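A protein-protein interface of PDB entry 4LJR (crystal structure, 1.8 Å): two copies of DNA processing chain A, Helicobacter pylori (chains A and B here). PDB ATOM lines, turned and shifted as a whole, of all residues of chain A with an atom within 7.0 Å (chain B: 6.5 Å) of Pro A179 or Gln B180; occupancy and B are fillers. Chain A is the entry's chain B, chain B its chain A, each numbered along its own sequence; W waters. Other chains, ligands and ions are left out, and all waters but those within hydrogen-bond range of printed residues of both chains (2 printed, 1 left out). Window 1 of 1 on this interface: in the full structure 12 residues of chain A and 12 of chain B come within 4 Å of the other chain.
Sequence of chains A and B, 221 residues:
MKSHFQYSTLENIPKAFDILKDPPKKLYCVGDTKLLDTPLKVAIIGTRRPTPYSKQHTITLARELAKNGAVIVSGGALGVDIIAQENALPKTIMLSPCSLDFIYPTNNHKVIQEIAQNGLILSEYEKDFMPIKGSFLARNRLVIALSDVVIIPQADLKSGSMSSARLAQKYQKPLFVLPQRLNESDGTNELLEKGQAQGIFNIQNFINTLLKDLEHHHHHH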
ATOM      1  N   TYR A  53      16.509  10.238 -11.291  1.00  0.00           N
ATOM      2  CA  TYR A  53      16.147   9.253 -10.277  1.00  0.00           C
ATOM      3  C   TYR A  53      14.849   8.519 -10.630  1.00  0.00           C
ATOM      4  O   TYR A  53      14.814   7.289 -10.689  1.00  0.00           O
ATOM      5  CB  TYR A  53      16.014   9.929  -8.912  1.00  0.00           C
ATOM      6  CG  TYR A  53      15.315   9.087  -7.871  1.00  0.00           C
ATOM      7  CD1 TYR A  53      15.986   8.064  -7.217  1.00  0.00           C
ATOM      8  CD2 TYR A  53      13.984   9.315  -7.541  1.00  0.00           C
ATOM      9  CE1 TYR A  53      15.353   7.290  -6.268  1.00  0.00           C
ATOM     10  CE2 TYR A  53      13.343   8.547  -6.590  1.00  0.00           C
ATOM     11  CZ  TYR A  53      14.034   7.535  -5.956  1.00  0.00           C
ATOM     12  OH  TYR A  53      13.410   6.763  -5.008  1.00  0.00           O
ATOM     13  N   SER A  54      13.779   9.275 -10.854  1.00  0.00           N
ATOM     14  CA  SER A  54      12.482   8.671 -11.140  1.00  0.00           C
ATOM     15  C   SER A  54      12.507   7.903 -12.454  1.00  0.00           C
ATOM     16  O   SER A  54      11.898   6.838 -12.577  1.00  0.00           O
ATOM     17  CB  SER A  54      11.381   9.733 -11.150  1.00  0.00           C
ATOM     18  OG  SER A  54      11.325  10.402  -9.902  1.00  0.00           O
ATOM     19  N   HIS A  57      14.222   4.257 -12.162  1.00  0.00           N
ATOM     20  CA  HIS A  57      13.378   3.271 -11.499  1.00  0.00           C
ATOM     21  C   HIS A  57      12.080   2.975 -12.260  1.00  0.00           C
ATOM     22  O   HIS A  57      11.547   1.869 -12.183  1.00  0.00           O
ATOM     23  CB  HIS A  57      13.108   3.685 -10.055  1.00  0.00           C
ATOM     24  CG  HIS A  57      14.341   3.717  -9.209  1.00  0.00           C
ATOM     25  ND1 HIS A  57      15.212   2.654  -9.130  1.00  0.00           N
ATOM     26  CD2 HIS A  57      14.855   4.688  -8.415  1.00  0.00           C
ATOM     27  CE1 HIS A  57      16.210   2.963  -8.318  1.00  0.00           C
ATOM     28  NE2 HIS A  57      16.015   4.189  -7.873  1.00  0.00           N
ATOM     29  N   PRO A 153       5.249   6.883 -10.030  1.00  0.00           N
ATOM     30  CA  PRO A 153       6.661   7.038  -9.650  1.00  0.00           C
ATOM     31  C   PRO A 153       6.990   8.418  -9.088  1.00  0.00           C
ATOM     32  O   PRO A 153       7.684   8.514  -8.071  1.00  0.00           O
ATOM     33  CB  PRO A 153       7.400   6.808 -10.967  1.00  0.00           C
ATOM     34  CG  PRO A 153       6.488   5.921 -11.751  1.00  0.00           C
ATOM     35  CD  PRO A 153       5.101   6.379 -11.408  1.00  0.00           C
ATOM     36  N   VAL A 177       3.780   4.196  -4.945  1.00  0.00           N
ATOM     37  CA  VAL A 177       4.660   5.267  -5.391  1.00  0.00           C
ATOM     38  C   VAL A 177       6.122   4.933  -5.132  1.00  0.00           C
ATOM     39  O   VAL A 177       6.429   3.976  -4.421  1.00  0.00           O
ATOM     40  CB  VAL A 177       4.319   6.597  -4.692  1.00  0.00           C
ATOM     41  CG1 VAL A 177       2.836   6.919  -4.863  1.00  0.00           C
ATOM     42  CG2 VAL A 177       4.696   6.536  -3.219  1.00  0.00           C
ATOM     43  N   LEU A 178       7.018   5.713  -5.734  1.00  0.00           N
ATOM     44  CA  LEU A 178       8.441   5.650  -5.404  1.00  0.00           C
ATOM     45  C   LEU A 178       8.707   6.567  -4.224  1.00  0.00           C
ATOM     46  O   LEU A 178       8.072   7.612  -4.100  1.00  0.00           O
ATOM     47  CB  LEU A 178       9.300   6.119  -6.579  1.00  0.00           C
ATOM     48  CG  LEU A 178       9.566   5.187  -7.759  1.00  0.00           C
ATOM     49  CD1 LEU A 178      10.425   5.899  -8.794  1.00  0.00           C
ATOM     50  CD2 LEU A 178      10.235   3.909  -7.288  1.00  0.00           C
ATOM     51  N   PRO A 179       9.639   6.176  -3.343  1.00  0.00           N
ATOM     52  CA  PRO A 179      10.107   7.094  -2.302  1.00  0.00           C
ATOM     53  C   PRO A 179      10.717   8.342  -2.934  1.00  0.00           C
ATOM     54  O   PRO A 179      11.491   8.235  -3.889  1.00  0.00           O
ATOM     55  CB  PRO A 179      11.190   6.283  -1.582  1.00  0.00           C
ATOM     56  CG  PRO A 179      10.827   4.857  -1.837  1.00  0.00           C
ATOM     57  CD  PRO A 179      10.251   4.843  -3.223  1.00  0.00           C
ATOM     58  N   GLN A 180      10.366   9.513  -2.411  1.00  0.00           N
ATOM     59  CA  GLN A 180      10.841  10.770  -2.975  1.00  0.00           C
ATOM     60  C   GLN A 180      11.263  11.737  -1.876  1.00  0.00           C
ATOM     61  O   GLN A 180      10.679  11.758  -0.794  1.00  0.00           O
ATOM     62  CB  GLN A 180       9.759  11.417  -3.845  1.00  0.00           C
ATOM     63  CG  GLN A 180       9.331  10.591  -5.053  1.00  0.00           C
ATOM     64  CD  GLN A 180      10.327  10.643  -6.195  1.00  0.00           C
ATOM     65  OE1 GLN A 180      11.422  11.185  -6.060  1.00  0.00           O
ATOM     66  NE2 GLN A 180       9.937  10.087  -7.343  1.00  0.00           N
ATOM     67  N   ARG A 181      12.280  12.541  -2.164  1.00  0.00           N
ATOM     68  CA  ARG A 181      12.765  13.526  -1.209  1.00  0.00           C
ATOM     69  C   ARG A 181      11.730  14.608  -0.929  1.00  0.00           C
ATOM     70  O   ARG A 181      10.786  14.800  -1.696  1.00  0.00           O
ATOM     71  CB  ARG A 181      14.062  14.166  -1.707  1.00  0.00           C
ATOM     72  CG  ARG A 181      15.260  13.236  -1.687  1.00  0.00           C
ATOM     73  CD  ARG A 181      16.509  13.935  -2.199  1.00  0.00           C
ATOM     74  NE  ARG A 181      17.670  13.052  -2.161  1.00  0.00           N
ATOM     75  CZ  ARG A 181      18.841  13.335  -2.722  1.00  0.00           C
ATOM     76  NH1 ARG A 181      19.005  14.478  -3.374  1.00  0.00           N
ATOM     77  NH2 ARG A 181      19.845  12.472  -2.636  1.00  0.00           N
ATOM     78  N   LEU A 182      11.920  15.312   0.180  1.00  0.00           N
ATOM     79  CA  LEU A 182      11.073  16.437   0.540  1.00  0.00           C
ATOM     80  C   LEU A 182      11.161  17.499  -0.553  1.00  0.00           C
ATOM     81  O   LEU A 182      12.256  17.919  -0.921  1.00  0.00           O
ATOM     82  CB  LEU A 182      11.540  17.017   1.877  1.00  0.00           C
ATOM     83  CG  LEU A 182      10.510  17.679   2.791  1.00  0.00           C
ATOM     84  CD1 LEU A 182       9.373  16.719   3.089  1.00  0.00           C
ATOM     85  CD2 LEU A 182      11.171  18.142   4.080  1.00  0.00           C
ATOM     86  N   SER A 185       8.426  15.795  -5.149  1.00  0.00           N
ATOM     87  CA  SER A 185       7.258  15.116  -5.672  1.00  0.00           C
ATOM     88  C   SER A 185       6.176  15.248  -4.616  1.00  0.00           C
ATOM     89  O   SER A 185       5.828  14.278  -3.949  1.00  0.00           O
ATOM     90  CB  SER A 185       7.590  13.644  -5.920  1.00  0.00           C
ATOM     91  OG  SER A 185       6.586  12.997  -6.680  1.00  0.00           O
ATOM     92  N   THR A 188       3.070  12.689  -4.764  1.00  0.00           N
ATOM     93  CA  THR A 188       3.201  11.317  -4.282  1.00  0.00           C
ATOM     94  C   THR A 188       3.462  11.290  -2.785  1.00  0.00           C
ATOM     95  O   THR A 188       2.972  10.414  -2.078  1.00  0.00           O
ATOM     96  CB  THR A 188       4.310  10.542  -5.026  1.00  0.00           C
ATOM     97  OG1 THR A 188       5.541  11.266  -4.945  1.00  0.00           O
ATOM     98  CG2 THR A 188       3.932  10.349  -6.493  1.00  0.00           C
ATOM     99  N   ASN A 189       4.228  12.261  -2.302  1.00  0.00           N
ATOM    100  CA  ASN A 189       4.510  12.342  -0.873  1.00  0.00           C
ATOM    101  C   ASN A 189       3.252  12.578  -0.039  1.00  0.00           C
ATOM    102  O   ASN A 189       3.110  12.027   1.052  1.00  0.00           O
ATOM    103  CB  ASN A 189       5.571  13.404  -0.587  1.00  0.00           C
ATOM    104  CG  ASN A 189       6.982  12.869  -0.742  1.00  0.00           C
ATOM    105  OD1 ASN A 189       7.214  11.664  -0.636  1.00  0.00           O
ATOM    106  ND2 ASN A 189       7.934  13.764  -0.992  1.00  0.00           N
ATOM    107  N   LEU A 192       1.529   9.382   0.356  1.00  0.00           N
ATOM    108  CA  LEU A 192       2.166   8.658   1.442  1.00  0.00           C
ATOM    109  C   LEU A 192       1.742   9.230   2.788  1.00  0.00           C
ATOM    110  O   LEU A 192       1.401   8.484   3.698  1.00  0.00           O
ATOM    111  CB  LEU A 192       3.689   8.701   1.310  1.00  0.00           C
ATOM    112  CG  LEU A 192       4.313   7.806   0.240  1.00  0.00           C
ATOM    113  CD1 LEU A 192       5.826   7.976   0.228  1.00  0.00           C
ATOM    114  CD2 LEU A 192       3.932   6.351   0.473  1.00  0.00           C
ATOM    115  N   GLY A 199       4.478   2.814  -0.517  1.00  0.00           N
ATOM    116  CA  GLY A 199       5.759   3.039  -1.157  1.00  0.00           C
ATOM    117  C   GLY A 199       6.374   1.762  -1.691  1.00  0.00           C
ATOM    118  O   GLY A 199       6.208   0.695  -1.101  1.00  0.00           O
ATOM    119  N   ILE A 200       7.072   1.867  -2.818  1.00  0.00           N
ATOM    120  CA  ILE A 200       7.856   0.754  -3.337  1.00  0.00           C
ATOM    121  C   ILE A 200       9.285   0.865  -2.816  1.00  0.00           C
ATOM    122  O   ILE A 200      10.066   1.678  -3.304  1.00  0.00           O
ATOM    123  CB  ILE A 200       7.871   0.731  -4.877  1.00  0.00           C
ATOM    124  CG1 ILE A 200       6.454   0.518  -5.416  1.00  0.00           C
ATOM    125  CG2 ILE A 200       8.798  -0.364  -5.383  1.00  0.00           C
ATOM    126  CD1 ILE A 200       6.334   0.669  -6.924  1.00  0.00           C
ATOM    127  N   PHE A 201       9.618   0.055  -1.816  1.00  0.00           N
ATOM    128  CA  PHE A 201      10.940   0.116  -1.192  1.00  0.00           C
ATOM    129  C   PHE A 201      11.879  -0.978  -1.699  1.00  0.00           C
ATOM    130  O   PHE A 201      13.060  -1.010  -1.350  1.00  0.00           O
ATOM    131  CB  PHE A 201      10.822   0.070   0.332  1.00  0.00           C
ATOM    132  CG  PHE A 201      10.125   1.263   0.920  1.00  0.00           C
ATOM    133  CD1 PHE A 201      10.823   2.433   1.173  1.00  0.00           C
ATOM    134  CD2 PHE A 201       8.773   1.217   1.217  1.00  0.00           C
ATOM    135  CE1 PHE A 201      10.184   3.535   1.708  1.00  0.00           C
ATOM    136  CE2 PHE A 201       8.129   2.315   1.755  1.00  0.00           C
ATOM    137  CZ  PHE A 201       8.837   3.476   2.002  1.00  0.00           C
ATOM    138  N   ASN A 202      11.343  -1.872  -2.521  1.00  0.00           N
ATOM    139  CA  ASN A 202      12.156  -2.866  -3.206  1.00  0.00           C
ATOM    140  C   ASN A 202      11.420  -3.423  -4.413  1.00  0.00           C
ATOM    141  O   ASN A 202      10.425  -4.130  -4.276  1.00  0.00           O
ATOM    142  CB  ASN A 202      12.569  -4.000  -2.270  1.00  0.00           C
ATOM    143  CG  ASN A 202      13.510  -4.983  -2.937  1.00  0.00           C
ATOM    144  OD1 ASN A 202      13.077  -5.962  -3.549  1.00  0.00           O
ATOM    145  ND2 ASN A 202      14.808  -4.719  -2.837  1.00  0.00           N
ATOM    146  N   THR B  51      24.034  13.361   3.315  1.00  0.00           N
ATOM    147  CA  THR B  51      24.030  14.030   2.023  1.00  0.00           C
ATOM    148  C   THR B  51      23.678  15.493   2.241  1.00  0.00           C
ATOM    149  O   THR B  51      23.124  15.845   3.273  1.00  0.00           O
ATOM    150  CB  THR B  51      22.941  13.435   1.123  1.00  0.00           C
ATOM    151  OG1 THR B  51      21.703  13.429   1.847  1.00  0.00           O
ATOM    152  CG2 THR B  51      23.293  12.010   0.734  1.00  0.00           C
ATOM    153  N   TYR B  53      21.244  17.023   1.041  1.00  0.00           N
ATOM    154  CA  TYR B  53      19.801  17.033   1.275  1.00  0.00           C
ATOM    155  C   TYR B  53      19.455  16.846   2.750  1.00  0.00           C
ATOM    156  O   TYR B  53      18.677  17.612   3.318  1.00  0.00           O
ATOM    157  CB  TYR B  53      19.115  15.943   0.444  1.00  0.00           C
ATOM    158  CG  TYR B  53      17.707  15.607   0.894  1.00  0.00           C
ATOM    159  CD1 TYR B  53      16.648  16.462   0.626  1.00  0.00           C
ATOM    160  CD2 TYR B  53      17.439  14.428   1.577  1.00  0.00           C
ATOM    161  CE1 TYR B  53      15.357  16.155   1.030  1.00  0.00           C
ATOM    162  CE2 TYR B  53      16.148  14.110   1.983  1.00  0.00           C
ATOM    163  CZ  TYR B  53      15.116  14.980   1.710  1.00  0.00           C
ATOM    164  OH  TYR B  53      13.836  14.665   2.114  1.00  0.00           O
ATOM    165  N   SER B  54      20.021  15.812   3.361  1.00  0.00           N
ATOM    166  CA  SER B  54      19.717  15.503   4.753  1.00  0.00           C
ATOM    167  C   SER B  54      20.245  16.583   5.682  1.00  0.00           C
ATOM    168  O   SER B  54      19.578  16.973   6.635  1.00  0.00           O
ATOM    169  CB  SER B  54      20.289  14.143   5.137  1.00  0.00           C
ATOM    170  OG  SER B  54      19.780  13.135   4.287  1.00  0.00           O
ATOM    171  N   ILE B 152      15.377  10.506  13.092  1.00  0.00           N
ATOM    172  CA  ILE B 152      16.532   9.993  12.367  1.00  0.00           C
ATOM    173  C   ILE B 152      16.464  10.456  10.908  1.00  0.00           C
ATOM    174  O   ILE B 152      15.812   9.819  10.084  1.00  0.00           O
ATOM    175  CB  ILE B 152      16.604   8.451  12.429  1.00  0.00           C
ATOM    176  CG1 ILE B 152      16.605   7.969  13.886  1.00  0.00           C
ATOM    177  CG2 ILE B 152      17.840   7.952  11.698  1.00  0.00           C
ATOM    178  CD1 ILE B 152      16.589   6.455  14.035  1.00  0.00           C
ATOM    179  N   PRO B 153      17.121  11.582  10.592  1.00  0.00           N
ATOM    180  CA  PRO B 153      17.110  12.160   9.239  1.00  0.00           C
ATOM    181  C   PRO B 153      17.609  11.189   8.171  1.00  0.00           C
ATOM    182  O   PRO B 153      16.970  11.047   7.125  1.00  0.00           O
ATOM    183  CB  PRO B 153      18.074  13.345   9.365  1.00  0.00           C
ATOM    184  CG  PRO B 153      17.969  13.743  10.793  1.00  0.00           C
ATOM    185  CD  PRO B 153      17.816  12.455  11.551  1.00  0.00           C
ATOM    186  N   GLN B 154      18.735  10.535   8.432  1.00  0.00           N
ATOM    187  CA  GLN B 154      19.333   9.608   7.475  1.00  0.00           C
ATOM    188  C   GLN B 154      20.150   8.545   8.209  1.00  0.00           C
ATOM    189  O   GLN B 154      20.826   8.848   9.190  1.00  0.00           O
ATOM    190  CB  GLN B 154      20.229  10.367   6.483  1.00  0.00           C
ATOM    191  CG  GLN B 154      20.843   9.484   5.410  1.00  0.00           C
ATOM    192  CD  GLN B 154      21.918  10.178   4.596  1.00  0.00           C
ATOM    193  OE1 GLN B 154      22.757   9.522   3.979  1.00  0.00           O
ATOM    194  NE2 GLN B 154      21.896  11.506   4.581  1.00  0.00           N
ATOM    195  N   ALA B 155      20.095   7.305   7.731  1.00  0.00           N
ATOM    196  CA  ALA B 155      20.828   6.217   8.370  1.00  0.00           C
ATOM    197  C   ALA B 155      20.926   4.964   7.504  1.00  0.00           C
ATOM    198  O   ALA B 155      19.976   4.602   6.800  1.00  0.00           O
ATOM    199  CB  ALA B 155      20.196   5.873   9.716  1.00  0.00           C
ATOM    200  N   VAL B 177      11.356  10.022  10.533  1.00  0.00           N
ATOM    201  CA  VAL B 177      12.485   9.999   9.621  1.00  0.00           C
ATOM    202  C   VAL B 177      12.214  10.944   8.451  1.00  0.00           C
ATOM    203  O   VAL B 177      11.058  11.254   8.150  1.00  0.00           O
ATOM    204  CB  VAL B 177      12.721   8.575   9.079  1.00  0.00           C
ATOM    205  CG1 VAL B 177      12.865   7.582  10.230  1.00  0.00           C
ATOM    206  CG2 VAL B 177      11.572   8.165   8.176  1.00  0.00           C
ATOM    207  N   LEU B 178      13.275  11.415   7.804  1.00  0.00           N
ATOM    208  CA  LEU B 178      13.128  12.198   6.583  1.00  0.00           C
ATOM    209  C   LEU B 178      12.789  11.271   5.438  1.00  0.00           C
ATOM    210  O   LEU B 178      13.304  10.155   5.374  1.00  0.00           O
ATOM    211  CB  LEU B 178      14.420  12.934   6.229  1.00  0.00           C
ATOM    212  CG  LEU B 178      14.824  14.201   6.979  1.00  0.00           C
ATOM    213  CD1 LEU B 178      16.040  14.805   6.298  1.00  0.00           C
ATOM    214  CD2 LEU B 178      13.682  15.201   7.015  1.00  0.00           C
ATOM    215  N   PRO B 179      11.921  11.729   4.522  1.00  0.00           N
ATOM    216  CA  PRO B 179      11.689  10.964   3.298  1.00  0.00           C
ATOM    217  C   PRO B 179      12.990  10.876   2.515  1.00  0.00           C
ATOM    218  O   PRO B 179      13.695  11.876   2.395  1.00  0.00           O
ATOM    219  CB  PRO B 179      10.672  11.819   2.534  1.00  0.00           C
ATOM    220  CG  PRO B 179      10.011  12.661   3.579  1.00  0.00           C
ATOM    221  CD  PRO B 179      11.075  12.931   4.604  1.00  0.00           C
ATOM    222  N   GLN B 180      13.296   9.692   1.995  1.00  0.00           N
ATOM    223  CA  GLN B 180      14.566   9.438   1.331  1.00  0.00           C
ATOM    224  C   GLN B 180      14.358   8.623   0.059  1.00  0.00           C
ATOM    225  O   GLN B 180      13.422   7.832  -0.037  1.00  0.00           O
ATOM    226  CB  GLN B 180      15.499   8.675   2.272  1.00  0.00           C
ATOM    227  CG  GLN B 180      15.929   9.450   3.498  1.00  0.00           C
ATOM    228  CD  GLN B 180      17.046  10.424   3.198  1.00  0.00           C
ATOM    229  OE1 GLN B 180      17.412  10.639   2.039  1.00  0.00           O
ATOM    230  NE2 GLN B 180      17.599  11.016   4.242  1.00  0.00           N
ATOM    231  N   ARG B 181      15.240   8.808  -0.916  1.00  0.00           N
ATOM    232  CA  ARG B 181      15.142   8.058  -2.157  1.00  0.00           C
ATOM    233  C   ARG B 181      15.454   6.587  -1.951  1.00  0.00           C
ATOM    234  O   ARG B 181      16.046   6.197  -0.942  1.00  0.00           O
ATOM    235  CB  ARG B 181      16.083   8.630  -3.212  1.00  0.00           C
ATOM    236  CG  ARG B 181      15.716  10.014  -3.664  1.00  0.00           C
ATOM    237  CD  ARG B 181      16.578  10.427  -4.834  1.00  0.00           C
ATOM    238  NE  ARG B 181      16.175  11.723  -5.357  1.00  0.00           N
ATOM    239  CZ  ARG B 181      16.964  12.500  -6.088  1.00  0.00           C
ATOM    240  NH1 ARG B 181      18.199  12.109  -6.368  1.00  0.00           N
ATOM    241  NH2 ARG B 181      16.522  13.669  -6.528  1.00  0.00           N
ATOM    242  N   LEU B 182      15.054   5.781  -2.926  1.00  0.00           N
ATOM    243  CA  LEU B 182      15.328   4.354  -2.932  1.00  0.00           C
ATOM    244  C   LEU B 182      16.831   4.093  -2.889  1.00  0.00           C
ATOM    245  O   LEU B 182      17.622   4.885  -3.403  1.00  0.00           O
ATOM    246  CB  LEU B 182      14.743   3.730  -4.196  1.00  0.00           C
ATOM    247  CG  LEU B 182      14.213   2.307  -4.071  1.00  0.00           C
ATOM    248  CD1 LEU B 182      13.134   2.268  -3.004  1.00  0.00           C
ATOM    249  CD2 LEU B 182      13.677   1.817  -5.409  1.00  0.00           C
ATOM    250  N   GLU B 184      18.990   4.624  -0.992  1.00  0.00           N
ATOM    251  CA  GLU B 184      19.748   5.519  -0.128  1.00  0.00           C
ATOM    252  C   GLU B 184      19.047   5.559   1.228  1.00  0.00           C
ATOM    253  O   GLU B 184      17.839   5.327   1.314  1.00  0.00           O
ATOM    254  CB  GLU B 184      19.866   6.923  -0.730  1.00  0.00           C
ATOM    255  CG  GLU B 184      18.819   7.921  -0.241  1.00  0.00           C
ATOM    256  CD  GLU B 184      18.869   9.244  -0.991  1.00  0.00           C
ATOM    257  OE1 GLU B 184      18.026  10.129  -0.704  1.00  0.00           O
ATOM    258  OE2 GLU B 184      19.745   9.395  -1.872  1.00  0.00           O
ATOM    259  N   SER B 185      19.808   5.835   2.282  1.00  0.00           N
ATOM    260  CA  SER B 185      19.272   5.821   3.640  1.00  0.00           C
ATOM    261  C   SER B 185      18.450   4.555   3.877  1.00  0.00           C
ATOM    262  O   SER B 185      17.264   4.624   4.210  1.00  0.00           O
ATOM    263  CB  SER B 185      18.419   7.064   3.896  1.00  0.00           C
ATOM    264  OG  SER B 185      18.279   7.299   5.289  1.00  0.00           O
ATOM    265  N   THR B 188      16.515   4.024   7.436  1.00  0.00           N
ATOM    266  CA  THR B 188      15.307   4.805   7.682  1.00  0.00           C
ATOM    267  C   THR B 188      14.159   4.396   6.762  1.00  0.00           C
ATOM    268  O   THR B 188      13.001   4.436   7.165  1.00  0.00           O
ATOM    269  CB  THR B 188      15.553   6.322   7.572  1.00  0.00           C
ATOM    270  OG1 THR B 188      15.897   6.665   6.225  1.00  0.00           O
ATOM    271  CG2 THR B 188      16.674   6.745   8.519  1.00  0.00           C
ATOM    272  N   ASN B 189      14.476   4.003   5.531  1.00  0.00           N
ATOM    273  CA  ASN B 189      13.438   3.518   4.625  1.00  0.00           C
ATOM    274  C   ASN B 189      12.828   2.194   5.087  1.00  0.00           C
ATOM    275  O   ASN B 189      11.635   1.955   4.904  1.00  0.00           O
ATOM    276  CB  ASN B 189      13.947   3.432   3.184  1.00  0.00           C
ATOM    277  CG  ASN B 189      13.888   4.770   2.471  1.00  0.00           C
ATOM    278  OD1 ASN B 189      13.185   5.683   2.903  1.00  0.00           O
ATOM    279  ND2 ASN B 189      14.623   4.892   1.371  1.00  0.00           N
ATOM    280  N   LEU B 192      10.278   3.035   7.616  1.00  0.00           N
ATOM    281  CA  LEU B 192       9.057   3.454   6.937  1.00  0.00           C
ATOM    282  C   LEU B 192       8.296   2.262   6.377  1.00  0.00           C
ATOM    283  O   LEU B 192       7.082   2.157   6.546  1.00  0.00           O
ATOM    284  CB  LEU B 192       9.373   4.427   5.799  1.00  0.00           C
ATOM    285  CG  LEU B 192       9.758   5.852   6.187  1.00  0.00           C
ATOM    286  CD1 LEU B 192      10.143   6.651   4.946  1.00  0.00           C
ATOM    287  CD2 LEU B 192       8.611   6.518   6.933  1.00  0.00           C
HETATM  288  O   HOH W   1      17.842  12.658  -9.751  1.00  0.00           O
HETATM  289  O   HOH W   2      18.296   5.234  -6.287  1.00  0.00           O
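Tyr A53 touches Arg B181 (CD1 to CD, 3.4 Å). Leu B182 touches His A57. Gln B180 touches Pro A179 (O to CB, 3.1 Å). O of Gln A180 touches CB of Pro B179 (3.3 Å). Arg A181 touches Tyr B53 (CB to CE1, 3.6 Å). Arg A181 touches Arg B181. Ile A200 touches Leu B182. Phe A201 touches Leu B182. Asn B189 touches Phe A201. Phe A201 touches Leu B192.
The backbone NH of Leu A182 lies within hydrogen-bond range of the side-chain hydroxyl of Tyr B53, 2.8 Å away. The backbone NH (N) of Leu B182 lies within hydrogen-bond range of the side-chain hydroxyl (OH) of Tyr A53. The guanidinium group (NH2) of Arg A181 is in salt-bridge range of the side-chain carboxylate (OE2) of Glu B184, at 3.2 Å.
The side-chain hydroxyl of Ser B54 lies within hydrogen-bond range of the side-chain amide nitrogen of Gln B180, 3.0 Å away. O of Pro B153 is in hydrogen-bond range of NE2 of Gln B180 (3.0 Å). The backbone NH of Arg B181 lies within hydrogen-bond range of the side-chain carboxylate of Glu B184, 3.1 Å away. O of Pro A153 is in hydrogen-bond range of NE2 of Gln A180 (2.8 Å). ND2 of Asn A189 is in hydrogen-bond range of O of Gln A180, at 3.4 Å. The side-chain amide nitrogen (ND2) of Asn A189 lies within hydrogen-bond range of the backbone carbonyl oxygen (O) of Arg A181 (3.1 Å).
Tyr A53 touches Arg B181, and with the chains exchanged Arg A181 touches Tyr B53. Tyr A53 touches Leu B182, and with the chains exchanged Leu A182 touches Tyr B53. Pro A179 touches Leu B182, but with the chains exchanged Leu A182 does not touch Pro B179 (4.1 Å). Arg A181 touches its own counterpart, Arg B181. 13 positions are printed for both chains.
Water W2 bridges a ring nitrogen (NE2) of His A57 (3.0 Å) and the backbone carbonyl oxygen of Leu B182 (3.0 Å). Water W1 bridges N of Tyr A53 (3.2 Å) and NH1 of Arg B181 (3.4 Å).
Of chain B, only Gln B180 and Leu B182 come within 4 Å of Pro A179. Gln B180 touches just one residue of chain A: Pro A179. Printed residues of chain B within 4 Å of Phe A201: Leu B182, Asn B189 and Leu B192. Printed residues of chain B within 4 Å of Ile A200: Leu B182. Of the printed residues of chain A, Pro B179 touches Gln A180 (3.3 Å). Of the printed residues of chain A, Glu B184 touches Arg A181. Of the printed residues of chain B, His A57 touches Leu B182 (3.9 Å). Ser A54 touches none of the printed residues of chain B. The nearest residue of chain B that does not touch Pro A179 is Arg B181 (4.04 Å). The nearest residue of chain A that does not touch Gln B180 is Gln A180 (4.2 Å).
Of the 18 printed residues of chain B, 8 touch a printed residue of chain A. Hydrophobic or aromatic side chains of chain B within 4 Å of the printed part of chain A: Tyr B53, Pro B179, Leu B182 and Leu B192. Among the printed residues, Asp or Glu carboxylates within 4 Å of a Lys or Arg side-chain nitrogen of the other chain: Arg A181 with Glu B184.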
